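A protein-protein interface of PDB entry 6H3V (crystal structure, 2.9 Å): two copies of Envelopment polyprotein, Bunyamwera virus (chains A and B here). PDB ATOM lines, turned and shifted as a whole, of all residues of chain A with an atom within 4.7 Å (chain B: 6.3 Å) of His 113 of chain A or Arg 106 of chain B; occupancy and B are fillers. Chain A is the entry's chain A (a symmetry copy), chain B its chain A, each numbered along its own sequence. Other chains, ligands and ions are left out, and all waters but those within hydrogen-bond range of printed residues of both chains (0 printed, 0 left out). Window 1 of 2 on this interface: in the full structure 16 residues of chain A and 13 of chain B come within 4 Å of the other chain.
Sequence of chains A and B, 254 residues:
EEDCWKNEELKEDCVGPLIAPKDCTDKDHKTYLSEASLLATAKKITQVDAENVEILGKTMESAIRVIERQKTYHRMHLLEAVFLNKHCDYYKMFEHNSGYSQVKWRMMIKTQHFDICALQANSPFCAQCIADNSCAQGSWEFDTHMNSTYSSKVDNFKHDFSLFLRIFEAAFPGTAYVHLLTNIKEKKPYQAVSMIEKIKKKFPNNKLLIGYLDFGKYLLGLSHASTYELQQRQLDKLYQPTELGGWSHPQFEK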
ATOM      1  N   ILE A 109      -0.019  33.577  23.865  1.00  0.00           N
ATOM      2  CA  ILE A 109      -1.021  34.332  24.621  1.00  0.00           C
ATOM      3  C   ILE A 109      -2.451  34.002  24.183  1.00  0.00           C
ATOM      4  O   ILE A 109      -3.382  34.146  24.982  1.00  0.00           O
ATOM      5  CB  ILE A 109      -0.790  35.854  24.570  1.00  0.00           C
ATOM      6  CG1 ILE A 109      -1.475  36.496  25.784  1.00  0.00           C
ATOM      7  CG2 ILE A 109      -1.410  36.458  23.310  1.00  0.00           C
ATOM      8  CD1 ILE A 109      -0.956  37.878  26.165  1.00  0.00           C
ATOM      9  N   LYS A 110      -2.674  33.553  22.940  1.00  0.00           N
ATOM     10  CA  LYS A 110      -4.068  33.350  22.546  1.00  0.00           C
ATOM     11  C   LYS A 110      -4.522  31.926  22.806  1.00  0.00           C
ATOM     12  O   LYS A 110      -5.710  31.629  22.637  1.00  0.00           O
ATOM     13  CB  LYS A 110      -4.309  33.720  21.061  1.00  0.00           C
ATOM     14  CG  LYS A 110      -4.083  35.215  20.698  1.00  0.00           C
ATOM     15  CD  LYS A 110      -5.090  36.176  21.354  1.00  0.00           C
ATOM     16  CE  LYS A 110      -5.947  36.902  20.322  1.00  0.00           C
ATOM     17  NZ  LYS A 110      -7.226  37.430  20.885  1.00  0.00           N
ATOM     18  N   THR A 111      -3.600  31.066  23.261  1.00  0.00           N
ATOM     19  CA  THR A 111      -3.822  29.633  23.429  1.00  0.00           C
ATOM     20  C   THR A 111      -3.788  29.220  24.896  1.00  0.00           C
ATOM     21  O   THR A 111      -4.750  28.633  25.406  1.00  0.00           O
ATOM     22  CB  THR A 111      -2.761  28.891  22.618  1.00  0.00           C
ATOM     23  OG1 THR A 111      -3.149  28.925  21.252  1.00  0.00           O
ATOM     24  CG2 THR A 111      -2.584  27.440  23.068  1.00  0.00           C
ATOM     25  N   GLN A 112      -2.663  29.459  25.568  1.00  0.00           N
ATOM     26  CA  GLN A 112      -2.564  29.332  27.013  1.00  0.00           C
ATOM     27  C   GLN A 112      -3.253  30.491  27.712  1.00  0.00           C
ATOM     28  O   GLN A 112      -2.905  31.659  27.492  1.00  0.00           O
ATOM     29  CB  GLN A 112      -1.100  29.314  27.410  1.00  0.00           C
ATOM     30  CG  GLN A 112      -0.290  28.538  26.455  1.00  0.00           C
ATOM     31  CD  GLN A 112      -0.405  27.095  26.744  1.00  0.00           C
ATOM     32  OE1 GLN A 112      -1.371  26.445  26.325  1.00  0.00           O
ATOM     33  NE2 GLN A 112       0.568  26.566  27.505  1.00  0.00           N
ATOM     34  N   HIS A 113      -4.176  30.168  28.608  1.00  0.00           N
ATOM     35  CA  HIS A 113      -5.021  31.162  29.243  1.00  0.00           C
ATOM     36  C   HIS A 113      -4.730  31.257  30.731  1.00  0.00           C
ATOM     37  O   HIS A 113      -4.247  30.309  31.353  1.00  0.00           O
ATOM     38  CB  HIS A 113      -6.489  30.837  28.999  1.00  0.00           C
ATOM     39  CG  HIS A 113      -6.882  30.955  27.557  1.00  0.00           C
ATOM     40  ND1 HIS A 113      -8.016  30.368  27.035  1.00  0.00           N
ATOM     41  CD2 HIS A 113      -6.286  31.602  26.531  1.00  0.00           C
ATOM     42  CE1 HIS A 113      -8.093  30.642  25.744  1.00  0.00           C
ATOM     43  NE2 HIS A 113      -7.059  31.393  25.415  1.00  0.00           N
ATOM     44  N   PHE A 114      -4.992  32.436  31.278  1.00  0.00           N
ATOM     45  CA  PHE A 114      -4.801  32.676  32.692  1.00  0.00           C
ATOM     46  C   PHE A 114      -5.962  32.133  33.508  1.00  0.00           C
ATOM     47  O   PHE A 114      -7.096  32.037  33.029  1.00  0.00           O
ATOM     48  CB  PHE A 114      -4.649  34.157  32.949  1.00  0.00           C
ATOM     49  CG  PHE A 114      -3.407  34.714  32.405  1.00  0.00           C
ATOM     50  CD1 PHE A 114      -2.197  34.456  33.029  1.00  0.00           C
ATOM     51  CD2 PHE A 114      -3.430  35.496  31.272  1.00  0.00           C
ATOM     52  CE1 PHE A 114      -1.012  34.967  32.526  1.00  0.00           C
ATOM     53  CE2 PHE A 114      -2.255  36.028  30.762  1.00  0.00           C
ATOM     54  CZ  PHE A 114      -1.038  35.758  31.390  1.00  0.00           C
ATOM     55  N   ASP A 115      -5.658  31.757  34.758  1.00  0.00           N
ATOM     56  CA  ASP A 115      -6.688  31.254  35.659  1.00  0.00           C
ATOM     57  C   ASP A 115      -7.618  32.365  36.112  1.00  0.00           C
ATOM     58  O   ASP A 115      -8.800  32.115  36.380  1.00  0.00           O
ATOM     59  CB  ASP A 115      -6.059  30.586  36.880  1.00  0.00           C
ATOM     60  CG  ASP A 115      -5.506  29.218  36.571  1.00  0.00           C
ATOM     61  OD1 ASP A 115      -5.922  28.625  35.536  1.00  0.00           O
ATOM     62  OD2 ASP A 115      -4.670  28.729  37.374  1.00  0.00           O
ATOM     63  N   HIS A 159       0.132  29.892  39.067  1.00  0.00           N
ATOM     64  CA  HIS A 159      -0.049  29.501  37.675  1.00  0.00           C
ATOM     65  C   HIS A 159      -0.013  30.705  36.762  1.00  0.00           C
ATOM     66  O   HIS A 159       0.610  30.669  35.693  1.00  0.00           O
ATOM     67  CB  HIS A 159      -1.366  28.771  37.491  1.00  0.00           C
ATOM     68  CG  HIS A 159      -1.685  28.479  36.064  1.00  0.00           C
ATOM     69  ND1 HIS A 159      -2.375  29.363  35.263  1.00  0.00           N
ATOM     70  CD2 HIS A 159      -1.399  27.406  35.288  1.00  0.00           C
ATOM     71  CE1 HIS A 159      -2.505  28.843  34.053  1.00  0.00           C
ATOM     72  NE2 HIS A 159      -1.926  27.653  34.044  1.00  0.00           N
ATOM     73  N   LEU A 163       2.812  31.565  33.971  1.00  0.00           N
ATOM     74  CA  LEU A 163       2.357  31.753  32.596  1.00  0.00           C
ATOM     75  C   LEU A 163       2.884  33.063  32.042  1.00  0.00           C
ATOM     76  O   LEU A 163       3.404  33.129  30.918  1.00  0.00           O
ATOM     77  CB  LEU A 163       0.829  31.724  32.524  1.00  0.00           C
ATOM     78  CG  LEU A 163       0.268  31.929  31.117  1.00  0.00           C
ATOM     79  CD1 LEU A 163       0.967  30.991  30.184  1.00  0.00           C
ATOM     80  CD2 LEU A 163      -1.245  31.697  31.039  1.00  0.00           C
ATOM     81  N   HIS B  96      -5.946  23.721  35.441  1.00  0.00           N
ATOM     82  CA  HIS B  96      -5.738  25.139  35.146  1.00  0.00           C
ATOM     83  C   HIS B  96      -6.020  25.410  33.669  1.00  0.00           C
ATOM     84  O   HIS B  96      -6.410  24.515  32.913  1.00  0.00           O
ATOM     85  CB  HIS B  96      -4.316  25.564  35.497  1.00  0.00           C
ATOM     86  CG  HIS B  96      -3.943  25.318  36.925  1.00  0.00           C
ATOM     87  ND1 HIS B  96      -3.859  26.331  37.860  1.00  0.00           N
ATOM     88  CD2 HIS B  96      -3.617  24.178  37.575  1.00  0.00           C
ATOM     89  CE1 HIS B  96      -3.495  25.822  39.022  1.00  0.00           C
ATOM     90  NE2 HIS B  96      -3.337  24.519  38.875  1.00  0.00           N
ATOM     91  N   ASN B  97      -5.823  26.666  33.251  1.00  0.00           N
ATOM     92  CA  ASN B  97      -6.142  27.080  31.887  1.00  0.00           C
ATOM     93  C   ASN B  97      -4.951  27.131  30.948  1.00  0.00           C
ATOM     94  O   ASN B  97      -5.127  27.463  29.777  1.00  0.00           O
ATOM     95  CB  ASN B  97      -6.837  28.428  31.905  1.00  0.00           C
ATOM     96  CG  ASN B  97      -8.184  28.329  32.530  1.00  0.00           C
ATOM     97  OD1 ASN B  97      -8.291  28.377  33.754  1.00  0.00           O
ATOM     98  ND2 ASN B  97      -9.225  28.103  31.707  1.00  0.00           N
ATOM     99  N   SER B  98      -3.752  26.846  31.418  1.00  0.00           N
ATOM    100  CA  SER B  98      -2.601  26.746  30.549  1.00  0.00           C
ATOM    101  C   SER B  98      -1.954  25.401  30.814  1.00  0.00           C
ATOM    102  O   SER B  98      -2.445  24.621  31.622  1.00  0.00           O
ATOM    103  CB  SER B  98      -1.621  27.893  30.785  1.00  0.00           C
ATOM    104  OG  SER B  98      -0.329  27.392  31.068  1.00  0.00           O
ATOM    105  N   GLY B  99      -0.925  25.076  30.056  1.00  0.00           N
ATOM    106  CA  GLY B  99      -0.009  24.012  30.425  1.00  0.00           C
ATOM    107  C   GLY B  99       0.528  23.320  29.190  1.00  0.00           C
ATOM    108  O   GLY B  99      -0.067  23.362  28.127  1.00  0.00           O
ATOM    109  N   GLN B 102      -1.727  20.853  27.519  1.00  0.00           N
ATOM    110  CA  GLN B 102      -2.905  21.418  26.891  1.00  0.00           C
ATOM    111  C   GLN B 102      -2.633  22.042  25.526  1.00  0.00           C
ATOM    112  O   GLN B 102      -3.590  22.245  24.765  1.00  0.00           O
ATOM    113  CB  GLN B 102      -3.548  22.439  27.832  1.00  0.00           C
ATOM    114  CG  GLN B 102      -4.005  21.834  29.179  1.00  0.00           C
ATOM    115  CD  GLN B 102      -5.131  22.645  29.845  1.00  0.00           C
ATOM    116  OE1 GLN B 102      -6.234  22.744  29.305  1.00  0.00           O
ATOM    117  NE2 GLN B 102      -4.848  23.233  31.010  1.00  0.00           N
ATOM    118  N   VAL B 103      -1.360  22.237  25.150  1.00  0.00           N
ATOM    119  CA  VAL B 103      -1.041  23.066  23.978  1.00  0.00           C
ATOM    120  C   VAL B 103      -1.791  22.594  22.735  1.00  0.00           C
ATOM    121  O   VAL B 103      -2.412  23.392  22.027  1.00  0.00           O
ATOM    122  CB  VAL B 103       0.479  23.102  23.729  1.00  0.00           C
ATOM    123  CG1 VAL B 103       0.762  23.753  22.393  1.00  0.00           C
ATOM    124  CG2 VAL B 103       1.173  23.905  24.813  1.00  0.00           C
ATOM    125  N   LYS B 104      -1.773  21.288  22.468  1.00  0.00           N
ATOM    126  CA  LYS B 104      -2.384  20.774  21.243  1.00  0.00           C
ATOM    127  C   LYS B 104      -3.877  21.091  21.170  1.00  0.00           C
ATOM    128  O   LYS B 104      -4.353  21.605  20.152  1.00  0.00           O
ATOM    129  CB  LYS B 104      -2.135  19.270  21.118  1.00  0.00           C
ATOM    130  CG  LYS B 104      -1.645  18.829  19.739  1.00  0.00           C
ATOM    131  CD  LYS B 104      -0.776  17.559  19.815  1.00  0.00           C
ATOM    132  CE  LYS B 104      -1.522  16.373  20.446  1.00  0.00           C
ATOM    133  NZ  LYS B 104      -0.679  15.139  20.531  1.00  0.00           N
ATOM    134  N   TRP B 105      -4.637  20.825  22.239  1.00  0.00           N
ATOM    135  CA  TRP B 105      -6.096  20.949  22.065  1.00  0.00           C
ATOM    136  C   TRP B 105      -6.570  22.411  22.096  1.00  0.00           C
ATOM    137  O   TRP B 105      -7.435  22.799  21.290  1.00  0.00           O
ATOM    138  CB  TRP B 105      -6.850  20.088  23.092  1.00  0.00           C
ATOM    139  CG  TRP B 105      -7.094  20.707  24.435  1.00  0.00           C
ATOM    140  CD1 TRP B 105      -6.287  20.628  25.543  1.00  0.00           C
ATOM    141  CD2 TRP B 105      -8.235  21.481  24.826  1.00  0.00           C
ATOM    142  NE1 TRP B 105      -6.848  21.322  26.586  1.00  0.00           N
ATOM    143  CE2 TRP B 105      -8.042  21.855  26.175  1.00  0.00           C
ATOM    144  CE3 TRP B 105      -9.394  21.906  24.167  1.00  0.00           C
ATOM    145  CZ2 TRP B 105      -8.970  22.630  26.874  1.00  0.00           C
ATOM    146  CZ3 TRP B 105     -10.308  22.685  24.862  1.00  0.00           C
ATOM    147  CH2 TRP B 105     -10.092  23.037  26.199  1.00  0.00           C
ATOM    148  N   ARG B 106      -5.985  23.249  22.968  1.00  0.00           N
ATOM    149  CA  ARG B 106      -6.365  24.657  22.979  1.00  0.00           C
ATOM    150  C   ARG B 106      -6.096  25.290  21.618  1.00  0.00           C
ATOM    151  O   ARG B 106      -6.979  25.942  21.045  1.00  0.00           O
ATOM    152  CB  ARG B 106      -5.645  25.445  24.084  1.00  0.00           C
ATOM    153  CG  ARG B 106      -5.252  24.693  25.338  1.00  0.00           C
ATOM    154  CD  ARG B 106      -6.162  24.865  26.558  1.00  0.00           C
ATOM    155  NE  ARG B 106      -6.597  26.234  26.829  1.00  0.00           N
ATOM    156  CZ  ARG B 106      -7.261  26.597  27.925  1.00  0.00           C
ATOM    157  NH1 ARG B 106      -7.655  27.842  28.083  1.00  0.00           N
ATOM    158  NH2 ARG B 106      -7.527  25.714  28.873  1.00  0.00           N
ATOM    159  N   MET B 107      -4.894  25.070  21.068  1.00  0.00           N
ATOM    160  CA  MET B 107      -4.572  25.554  19.724  1.00  0.00           C
ATOM    161  C   MET B 107      -5.639  25.106  18.747  1.00  0.00           C
ATOM    162  O   MET B 107      -6.254  25.926  18.042  1.00  0.00           O
ATOM    163  CB  MET B 107      -3.201  25.035  19.282  1.00  0.00           C
ATOM    164  CG  MET B 107      -2.327  26.053  18.546  1.00  0.00           C
ATOM    165  SD  MET B 107      -0.528  25.912  18.858  1.00  0.00           S
ATOM    166  CE  MET B 107      -0.230  24.195  18.405  1.00  0.00           C
ATOM    167  N   MET B 108      -5.945  23.805  18.769  1.00  0.00           N
ATOM    168  CA  MET B 108      -6.962  23.299  17.862  1.00  0.00           C
ATOM    169  C   MET B 108      -8.307  23.982  18.118  1.00  0.00           C
ATOM    170  O   MET B 108      -8.907  24.543  17.193  1.00  0.00           O
ATOM    171  CB  MET B 108      -7.057  21.782  17.981  1.00  0.00           C
ATOM    172  CG  MET B 108      -7.802  21.174  16.825  1.00  0.00           C
ATOM    173  SD  MET B 108      -7.826  19.378  16.888  1.00  0.00           S
ATOM    174  CE  MET B 108      -6.049  19.101  16.784  1.00  0.00           C
ATOM    175  N   ILE B 109      -8.750  24.051  19.383  1.00  0.00           N
ATOM    176  CA  ILE B 109     -10.078  24.630  19.597  1.00  0.00           C
ATOM    177  C   ILE B 109     -10.135  26.112  19.212  1.00  0.00           C
ATOM    178  O   ILE B 109     -11.212  26.610  18.870  1.00  0.00           O
ATOM    179  CB  ILE B 109     -10.592  24.437  21.037  1.00  0.00           C
ATOM    180  CG1 ILE B 109     -12.124  24.535  21.029  1.00  0.00           C
ATOM    181  CG2 ILE B 109     -10.059  25.534  21.959  1.00  0.00           C
ATOM    182  CD1 ILE B 109     -12.820  23.898  22.226  1.00  0.00           C
ATOM    183  N   LYS B 110      -9.016  26.846  19.245  1.00  0.00           N
ATOM    184  CA  LYS B 110      -9.148  28.275  18.964  1.00  0.00           C
ATOM    185  C   LYS B 110      -8.934  28.580  17.493  1.00  0.00           C
ATOM    186  O   LYS B 110      -9.131  29.728  17.078  1.00  0.00           O
ATOM    187  CB  LYS B 110      -8.184  29.127  19.827  1.00  0.00           C
ATOM    188  CG  LYS B 110      -8.434  29.072  21.361  1.00  0.00           C
ATOM    189  CD  LYS B 110      -9.769  29.698  21.800  1.00  0.00           C
ATOM    190  CE  LYS B 110      -9.567  30.912  22.702  1.00  0.00           C
ATOM    191  NZ  LYS B 110     -10.748  31.825  22.735  1.00  0.00           N
ATOM    192  N   THR B 111      -8.583  27.556  16.704  1.00  0.00           N
ATOM    193  CA  THR B 111      -8.199  27.690  15.302  1.00  0.00           C
ATOM    194  C   THR B 111      -9.211  27.033  14.369  1.00  0.00           C
ATOM    195  O   THR B 111      -9.753  27.687  13.470  1.00  0.00           O
ATOM    196  CB  THR B 111      -6.808  27.080  15.131  1.00  0.00           C
ATOM    197  OG1 THR B 111      -5.856  28.015  15.619  1.00  0.00           O
ATOM    198  CG2 THR B 111      -6.492  26.734  13.676  1.00  0.00           C
ATOM    199  N   ASN B 133     -13.851  33.402  25.547  1.00  0.00           N
ATOM    200  CA  ASN B 133     -13.082  32.495  26.403  1.00  0.00           C
ATOM    201  C   ASN B 133     -13.525  32.563  27.870  1.00  0.00           C
ATOM    202  O   ASN B 133     -12.960  31.841  28.710  1.00  0.00           O
ATOM    203  CB  ASN B 133     -11.558  32.692  26.222  1.00  0.00           C
ATOM    204  CG  ASN B 133     -10.854  33.332  27.426  1.00  0.00           C
ATOM    205  OD1 ASN B 133     -11.337  34.290  28.030  1.00  0.00           O
ATOM    206  ND2 ASN B 133      -9.678  32.806  27.755  1.00  0.00           N
ATOM    207  N   ASN B 206     -11.183  24.689  34.478  1.00  0.00           N
ATOM    208  CA  ASN B 206     -10.697  24.832  33.122  1.00  0.00           C
ATOM    209  C   ASN B 206     -11.930  25.192  32.311  1.00  0.00           C
ATOM    210  O   ASN B 206     -12.579  24.339  31.705  1.00  0.00           O
ATOM    211  CB  ASN B 206     -10.079  23.499  32.717  1.00  0.00           C
ATOM    212  CG  ASN B 206      -9.265  23.563  31.478  1.00  0.00           C
ATOM    213  OD1 ASN B 206      -9.433  24.440  30.635  1.00  0.00           O
ATOM    214  ND2 ASN B 206      -8.382  22.594  31.338  1.00  0.00           N
ATOM    215  N   LYS B 207     -12.181  26.487  32.161  1.00  0.00           N
ATOM    216  CA  LYS B 207     -13.524  26.860  31.721  1.00  0.00           C
ATOM    217  C   LYS B 207     -13.720  26.543  30.252  1.00  0.00           C
ATOM    218  O   LYS B 207     -14.759  25.985  29.875  1.00  0.00           O
ATOM    219  CB  LYS B 207     -13.816  28.326  31.994  1.00  0.00           C
ATOM    220  CG  LYS B 207     -13.806  28.679  33.462  1.00  0.00           C
ATOM    221  CD  LYS B 207     -14.724  27.811  34.298  1.00  0.00           C
ATOM    222  CE  LYS B 207     -14.941  28.472  35.653  1.00  0.00           C
ATOM    223  NZ  LYS B 207     -15.392  27.494  36.663  1.00  0.00           N
ATOM    224  N   LEU B 208     -12.726  26.870  29.418  1.00  0.00           N
ATOM    225  CA  LEU B 208     -12.743  26.418  28.029  1.00  0.00           C
ATOM    226  C   LEU B 208     -13.027  24.922  27.951  1.00  0.00           C
ATOM    227  O   LEU B 208     -13.882  24.472  27.176  1.00  0.00           O
ATOM    228  CB  LEU B 208     -11.409  26.740  27.364  1.00  0.00           C
ATOM    229  CG  LEU B 208     -11.465  26.861  25.848  1.00  0.00           C
ATOM    230  CD1 LEU B 208     -12.422  27.987  25.517  1.00  0.00           C
ATOM    231  CD2 LEU B 208     -10.085  27.135  25.278  1.00  0.00           C
ATOM    232  N   LEU B 209     -12.337  24.137  28.776  1.00  0.00           N
ATOM    233  CA  LEU B 209     -12.505  22.695  28.700  1.00  0.00           C
ATOM    234  C   LEU B 209     -13.942  22.309  29.003  1.00  0.00           C
ATOM    235  O   LEU B 209     -14.580  21.593  28.220  1.00  0.00           O
ATOM    236  CB  LEU B 209     -11.544  21.998  29.661  1.00  0.00           C
ATOM    237  CG  LEU B 209     -11.615  20.470  29.609  1.00  0.00           C
ATOM    238  CD1 LEU B 209     -11.049  19.986  28.287  1.00  0.00           C
ATOM    239  CD2 LEU B 209     -10.930  19.823  30.824  1.00  0.00           C
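His 113 of chain A touches just these residues of chain B: Asn 97, Ser 98, Arg 106, Lys 110 and Asn 133. Arg 106 of chain B touches just these residues of chain A: Thr 111 and His 113. Of the printed residues of chain A, Gly 99 of chain B touches Gln 112 (3.3 Å). Printed residues of chain A within 4 Å of Asn 97 of chain B: His 113 (3.1 Å), Phe 114 (3.8 Å) and Asp 115 (3.0 Å). Printed residues of chain B within 4 Å of Phe 114 of chain A: Asn 97. The nearest residue of chain B that does not touch His 113 of chain A is Leu 208 of chain B (4.1 Å). The nearest printed residue of chain B that does not touch Leu 163 of chain A is Asn 97 of chain B (5.9 Å).
The side-chain amide nitrogen (NE2) of Gln 102 of chain B lies within hydrogen-bond range of the backbone carbonyl oxygen (O) of His 96 of chain B (2.8 Å). NH1 of Arg 106 of chain B sits close to O of Asn 97 of chain B. The backbone carbonyl oxygen (O) of Ser 98 of chain B sits at hydrogen-bond distance from the side-chain amide nitrogen (NE2) of Gln 102 of chain B, 2.8 Å away. The side-chain amide oxygen (OE1) of Gln 102 of chain B sits at hydrogen-bond distance from the guanidinium group (NH2) of Arg 106 of chain B, 3.3 Å away. The backbone carbonyl oxygen (O) of Lys 110 of chain A lies within hydrogen-bond range of a ring nitrogen (NE2) of His 113 of chain A, at 3.1 Å. OD2 of Asp 115 of chain A is in hydrogen-bond range of ND1 of His 159 of chain A, at 3.2 Å.
CE of Lys 110 of chain B touches O of Lys 110 of chain A (3.9 Å). N of Met 107 of chain B touches CG2 of Thr 111 of chain A (3.9 Å). Ser 98 of chain B touches Gln 112 of chain A. Gln 112 of chain A touches Val 103 of chain B (NE2 to CG2, 3.8 Å). CE of Lys 110 of chain B touches CE1 of His 113 of chain A, 3.4 Å away. Asn 97 of chain B touches Phe 114 of chain A. CB of His 96 of chain B touches CD2 of His 159 of chain A (3.5 Å). Leu 163 of chain A touches Ser 98 of chain B (CD2 to CB, 3.8 Å).
Of the 19 printed residues of chain B, 9 touch a printed residue of chain A. Hydrophobic or aromatic side chains of chain B within 4 Å of the printed part of chain A: His 96 and Val 103. Hydrophobic or aromatic side chains of chain A within 4 Å of the printed part of chain B: His 113, His 159 and Leu 163. Among the printed residues, 17 pairs touch across the chains. Among the printed residues, no Asp or Glu carboxylate lies within 4 Å of a Lys or Arg side-chain nitrogen of the other chain.
ND1 of His 96 of chain B sits at hydrogen-bond distance from OD2 of Asp 115 of chain A. N of His 113 of chain A sits at hydrogen-bond distance from O of Asn 97 of chain B, 3.1 Å away. The side-chain amide oxygen (OD1) of Asn 97 of chain B sits close to the side-chain carboxylate (OD1) of Asp 115 of chain A (3.0 Å). N of Ser 98 of chain B lies within hydrogen-bond range of O of His 113 of chain A, 3.5 Å away. The backbone NH of Ser 98 of chain B sits close to a ring nitrogen (NE2) of His 159 of chain A (3.3 Å). The backbone NH of Gly 99 of chain B sits close to the side-chain amide nitrogen of Gln 112 of chain A (3.3 Å). O of Thr 111 of chain A sits at hydrogen-bond distance from NE of Arg 106 of chain B (3.3 Å). A ring nitrogen (ND1) of His 113 of chain A lies within hydrogen-bond range of the guanidinium group of Arg 106 of chain B (2.8 Å). ND1 of His 113 of chain A lies within hydrogen-bond range of ND2 of Asn 133 of chain B, 3.0 Å away.
Lys 110 of chain A touches its own counterpart, Lys 110 of chain B. 3 positions are printed for both chains.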
